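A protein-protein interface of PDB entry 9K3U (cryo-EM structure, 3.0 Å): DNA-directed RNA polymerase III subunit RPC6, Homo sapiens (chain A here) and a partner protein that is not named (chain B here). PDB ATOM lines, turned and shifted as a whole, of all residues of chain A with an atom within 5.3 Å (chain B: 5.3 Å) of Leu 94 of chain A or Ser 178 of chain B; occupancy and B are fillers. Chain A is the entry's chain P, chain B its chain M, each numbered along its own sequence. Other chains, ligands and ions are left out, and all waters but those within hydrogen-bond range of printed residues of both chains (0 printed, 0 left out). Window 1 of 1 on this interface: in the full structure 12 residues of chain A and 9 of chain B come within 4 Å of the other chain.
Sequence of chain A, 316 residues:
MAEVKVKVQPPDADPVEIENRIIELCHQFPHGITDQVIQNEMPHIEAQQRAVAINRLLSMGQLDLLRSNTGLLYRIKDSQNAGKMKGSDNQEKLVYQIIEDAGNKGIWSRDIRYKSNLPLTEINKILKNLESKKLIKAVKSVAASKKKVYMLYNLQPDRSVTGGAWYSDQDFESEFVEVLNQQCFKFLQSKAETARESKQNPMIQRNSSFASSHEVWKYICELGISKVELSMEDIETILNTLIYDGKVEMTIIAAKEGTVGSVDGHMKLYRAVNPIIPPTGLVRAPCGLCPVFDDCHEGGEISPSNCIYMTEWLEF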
ATOM      1  N   ASP A  89      -2.032  -4.034  -4.285  1.00  0.00           N
ATOM      2  CA  ASP A  89      -1.949  -5.359  -3.679  1.00  0.00           C
ATOM      3  C   ASP A  89      -0.723  -6.129  -4.155  1.00  0.00           C
ATOM      4  O   ASP A  89      -0.384  -7.160  -3.560  1.00  0.00           O
ATOM      5  CB  ASP A  89      -3.219  -6.152  -3.988  1.00  0.00           C
ATOM      6  CG  ASP A  89      -3.181  -7.564  -3.436  1.00  0.00           C
ATOM      7  OD1 ASP A  89      -3.282  -7.723  -2.201  1.00  0.00           O
ATOM      8  OD2 ASP A  89      -3.048  -8.513  -4.234  1.00  0.00           O
ATOM      9  N   ASN A  90      -0.054  -5.652  -5.206  1.00  0.00           N
ATOM     10  CA  ASN A  90       1.114  -6.356  -5.727  1.00  0.00           C
ATOM     11  C   ASN A  90       2.183  -6.514  -4.651  1.00  0.00           C
ATOM     12  O   ASN A  90       2.585  -7.633  -4.323  1.00  0.00           O
ATOM     13  CB  ASN A  90       1.673  -5.618  -6.942  1.00  0.00           C
ATOM     14  CG  ASN A  90       0.707  -5.606  -8.112  1.00  0.00           C
ATOM     15  OD1 ASN A  90      -0.112  -6.514  -8.263  1.00  0.00           O
ATOM     16  ND2 ASN A  90       0.797  -4.580  -8.947  1.00  0.00           N
ATOM     17  N   GLN A  91       2.655  -5.397  -4.092  1.00  0.00           N
ATOM     18  CA  GLN A  91       3.669  -5.475  -3.041  1.00  0.00           C
ATOM     19  C   GLN A  91       3.116  -6.129  -1.783  1.00  0.00           C
ATOM     20  O   GLN A  91       3.841  -6.852  -1.086  1.00  0.00           O
ATOM     21  CB  GLN A  91       4.206  -4.080  -2.722  1.00  0.00           C
ATOM     22  CG  GLN A  91       5.138  -3.508  -3.783  1.00  0.00           C
ATOM     23  CD  GLN A  91       4.436  -3.231  -5.099  1.00  0.00           C
ATOM     24  OE1 GLN A  91       3.209  -3.264  -5.180  1.00  0.00           O
ATOM     25  NE2 GLN A  91       5.217  -2.955  -6.138  1.00  0.00           N
ATOM     26  N   GLU A  92       1.840  -5.892  -1.475  1.00  0.00           N
ATOM     27  CA  GLU A  92       1.215  -6.553  -0.335  1.00  0.00           C
ATOM     28  C   GLU A  92       1.434  -8.060  -0.396  1.00  0.00           C
ATOM     29  O   GLU A  92       1.994  -8.659   0.531  1.00  0.00           O
ATOM     30  CB  GLU A  92      -0.278  -6.223  -0.302  1.00  0.00           C
ATOM     31  CG  GLU A  92      -1.034  -6.850   0.854  1.00  0.00           C
ATOM     32  CD  GLU A  92      -2.506  -6.499   0.831  1.00  0.00           C
ATOM     33  OE1 GLU A  92      -2.998  -6.048  -0.224  1.00  0.00           O
ATOM     34  OE2 GLU A  92      -3.173  -6.668   1.873  1.00  0.00           O
ATOM     35  N   LYS A  93       1.006  -8.690  -1.493  1.00  0.00           N
ATOM     36  CA  LYS A  93       1.163 -10.137  -1.615  1.00  0.00           C
ATOM     37  C   LYS A  93       2.622 -10.530  -1.814  1.00  0.00           C
ATOM     38  O   LYS A  93       3.047 -11.583  -1.321  1.00  0.00           O
ATOM     39  CB  LYS A  93       0.295 -10.671  -2.758  1.00  0.00           C
ATOM     40  CG  LYS A  93       0.559 -10.053  -4.124  1.00  0.00           C
ATOM     41  CD  LYS A  93       1.570 -10.854  -4.933  1.00  0.00           C
ATOM     42  CE  LYS A  93       1.816 -10.221  -6.293  1.00  0.00           C
ATOM     43  NZ  LYS A  93       2.818 -10.979  -7.093  1.00  0.00           N
ATOM     44  N   LEU A  94       3.406  -9.704  -2.505  1.00  0.00           N
ATOM     45  CA  LEU A  94       4.814  -9.987  -2.750  1.00  0.00           C
ATOM     46  C   LEU A  94       5.671  -9.821  -1.506  1.00  0.00           C
ATOM     47  O   LEU A  94       6.886 -10.011  -1.581  1.00  0.00           O
ATOM     48  CB  LEU A  94       5.339  -9.081  -3.867  1.00  0.00           C
ATOM     49  CG  LEU A  94       6.580  -9.571  -4.613  1.00  0.00           C
ATOM     50  CD1 LEU A  94       6.268 -10.849  -5.377  1.00  0.00           C
ATOM     51  CD2 LEU A  94       7.103  -8.494  -5.552  1.00  0.00           C
ATOM     52  N   VAL A  95       5.075  -9.407  -0.393  1.00  0.00           N
ATOM     53  CA  VAL A  95       5.705  -9.472   0.921  1.00  0.00           C
ATOM     54  C   VAL A  95       5.067 -10.559   1.784  1.00  0.00           C
ATOM     55  O   VAL A  95       5.763 -11.319   2.467  1.00  0.00           O
ATOM     56  CB  VAL A  95       5.645  -8.097   1.625  1.00  0.00           C
ATOM     57  CG1 VAL A  95       6.223  -8.187   3.029  1.00  0.00           C
ATOM     58  CG2 VAL A  95       6.381  -7.046   0.804  1.00  0.00           C
ATOM     59  N   TYR A  96       3.733 -10.654   1.751  1.00  0.00           N
ATOM     60  CA  TYR A  96       3.038 -11.684   2.507  1.00  0.00           C
ATOM     61  C   TYR A  96       3.487 -13.081   2.110  1.00  0.00           C
ATOM     62  O   TYR A  96       3.411 -13.999   2.931  1.00  0.00           O
ATOM     63  CB  TYR A  96       1.527 -11.548   2.313  1.00  0.00           C
ATOM     64  CG  TYR A  96       0.714 -12.396   3.267  1.00  0.00           C
ATOM     65  CD1 TYR A  96       0.371 -11.924   4.527  1.00  0.00           C
ATOM     66  CD2 TYR A  96       0.289 -13.669   2.908  1.00  0.00           C
ATOM     67  CE1 TYR A  96      -0.368 -12.694   5.403  1.00  0.00           C
ATOM     68  CE2 TYR A  96      -0.453 -14.446   3.775  1.00  0.00           C
ATOM     69  CZ  TYR A  96      -0.779 -13.954   5.022  1.00  0.00           C
ATOM     70  OH  TYR A  96      -1.517 -14.724   5.892  1.00  0.00           O
ATOM     71  N   GLN A  97       3.972 -13.260   0.880  1.00  0.00           N
ATOM     72  CA  GLN A  97       4.467 -14.569   0.463  1.00  0.00           C
ATOM     73  C   GLN A  97       5.537 -15.080   1.424  1.00  0.00           C
ATOM     74  O   GLN A  97       5.367 -16.120   2.068  1.00  0.00           O
ATOM     75  CB  GLN A  97       5.014 -14.490  -0.964  1.00  0.00           C
ATOM     76  CG  GLN A  97       4.061 -15.016  -2.024  1.00  0.00           C
ATOM     77  CD  GLN A  97       4.636 -14.906  -3.424  1.00  0.00           C
ATOM     78  OE1 GLN A  97       5.724 -14.366  -3.618  1.00  0.00           O
ATOM     79  NE2 GLN A  97       3.907 -15.422  -4.406  1.00  0.00           N
ATOM     80  N   SER A 116      12.950  -8.644  -0.368  1.00  0.00           N
ATOM     81  CA  SER A 116      12.009  -7.887  -1.179  1.00  0.00           C
ATOM     82  C   SER A 116      12.689  -6.923  -2.141  1.00  0.00           C
ATOM     83  O   SER A 116      12.073  -6.533  -3.140  1.00  0.00           O
ATOM     84  CB  SER A 116      11.050  -7.100  -0.279  1.00  0.00           C
ATOM     85  OG  SER A 116      11.756  -6.189   0.542  1.00  0.00           O
ATOM     86  N   ARG B 176       9.076 -18.379  -4.622  1.00  0.00           N
ATOM     87  CA  ARG B 176      10.008 -17.288  -4.386  1.00  0.00           C
ATOM     88  C   ARG B 176       9.423 -15.968  -4.869  1.00  0.00           C
ATOM     89  O   ARG B 176       8.498 -15.933  -5.687  1.00  0.00           O
ATOM     90  CB  ARG B 176      11.337 -17.553  -5.098  1.00  0.00           C
ATOM     91  CG  ARG B 176      12.057 -18.801  -4.623  1.00  0.00           C
ATOM     92  CD  ARG B 176      13.386 -18.983  -5.339  1.00  0.00           C
ATOM     93  NE  ARG B 176      14.099 -20.172  -4.878  1.00  0.00           N
ATOM     94  CZ  ARG B 176      15.288 -20.556  -5.332  1.00  0.00           C
ATOM     95  NH1 ARG B 176      15.912 -19.846  -6.262  1.00  0.00           N
ATOM     96  NH2 ARG B 176      15.856 -21.654  -4.849  1.00  0.00           N
ATOM     97  N   PHE B 177       9.969 -14.875  -4.345  1.00  0.00           N
ATOM     98  CA  PHE B 177       9.508 -13.550  -4.734  1.00  0.00           C
ATOM     99  C   PHE B 177       9.964 -13.214  -6.145  1.00  0.00           C
ATOM    100  O   PHE B 177      11.116 -13.454  -6.517  1.00  0.00           O
ATOM    101  CB  PHE B 177      10.037 -12.494  -3.760  1.00  0.00           C
ATOM    102  CG  PHE B 177       9.384 -12.516  -2.406  1.00  0.00           C
ATOM    103  CD1 PHE B 177       8.308 -13.348  -2.138  1.00  0.00           C
ATOM    104  CD2 PHE B 177       9.846 -11.687  -1.399  1.00  0.00           C
ATOM    105  CE1 PHE B 177       7.718 -13.352  -0.895  1.00  0.00           C
ATOM    106  CE2 PHE B 177       9.258 -11.688  -0.154  1.00  0.00           C
ATOM    107  CZ  PHE B 177       8.191 -12.521   0.097  1.00  0.00           C
ATOM    108  N   SER B 178       9.046 -12.656  -6.938  1.00  0.00           N
ATOM    109  CA  SER B 178       9.396 -12.036  -8.214  1.00  0.00           C
ATOM    110  C   SER B 178       9.994 -10.658  -7.920  1.00  0.00           C
ATOM    111  O   SER B 178       9.442  -9.609  -8.254  1.00  0.00           O
ATOM    112  CB  SER B 178       8.177 -11.944  -9.120  1.00  0.00           C
ATOM    113  OG  SER B 178       7.161 -11.152  -8.529  1.00  0.00           O
ATOM    114  N   ARG B 179      11.151 -10.686  -7.266  1.00  0.00           N
ATOM    115  CA  ARG B 179      11.764  -9.462  -6.779  1.00  0.00           C
ATOM    116  C   ARG B 179      11.975  -8.486  -7.936  1.00  0.00           C
ATOM    117  O   ARG B 179      12.295  -8.910  -9.053  1.00  0.00           O
ATOM    118  CB  ARG B 179      13.104  -9.766  -6.106  1.00  0.00           C
ATOM    119  CG  ARG B 179      13.030 -10.782  -4.976  1.00  0.00           C
ATOM    120  CD  ARG B 179      14.417 -11.117  -4.451  1.00  0.00           C
ATOM    121  NE  ARG B 179      14.393 -12.190  -3.460  1.00  0.00           N
ATOM    122  CZ  ARG B 179      15.477 -12.707  -2.887  1.00  0.00           C
ATOM    123  NH1 ARG B 179      16.683 -12.253  -3.205  1.00  0.00           N
ATOM    124  NH2 ARG B 179      15.355 -13.681  -1.997  1.00  0.00           N
ATOM    125  N   PRO B 180      11.805  -7.180  -7.711  1.00  0.00           N
ATOM    126  CA  PRO B 180      12.100  -6.219  -8.782  1.00  0.00           C
ATOM    127  C   PRO B 180      13.578  -6.224  -9.134  1.00  0.00           C
ATOM    128  O   PRO B 180      14.416  -5.799  -8.335  1.00  0.00           O
ATOM    129  CB  PRO B 180      11.655  -4.878  -8.189  1.00  0.00           C
ATOM    130  CG  PRO B 180      11.728  -5.073  -6.714  1.00  0.00           C
ATOM    131  CD  PRO B 180      11.374  -6.510  -6.472  1.00  0.00           C
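Leu 94 of chain A touches two residues of chain B.
Of chain A, only Leu 94 (3.3 Å) comes within 4 Å of Ser 178 of chain B.
Printed residues of chain A within 4 Å of Phe 177 of chain B: Leu 94, Val 95 and Gln 97.
Of the printed residues of chain A, Pro 180 of chain B touches Ser 116 (3.4 Å).
Of the printed residues of chain B, Gln 97 of chain A touches Arg 176 and Phe 177.
The nearest residue of chain A that does not touch Ser 178 of chain B is Lys 93 of chain A (4.6 Å).
The nearest printed residue of chain B that does not touch Val 95 of chain A is Ser 178 of chain B (8.3 Å).
Hydrophobic or aromatic side chains of chain B that line the printed part of chain A: Phe 177 and Pro 180.
Along chain A the printed residues that touch a printed residue of chain B span positions 94 to 116.
Leu 94 of chain A touches Phe 177 of chain B (O to CE2, 3.2 Å).
Ser 178 of chain B touches Leu 94 of chain A (OG to CD1, 3.3 Å).
O of Val 95 of chain A touches CZ of Phe 177 of chain B (3.6 Å).
OE1 of Gln 97 of chain A touches O of Arg 176 of chain B (3.8 Å).
CE1 of Phe 177 of chain B touches CB of Gln 97 of chain A, 2.9 Å away.
Pro 180 of chain B touches Ser 116 of chain A.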
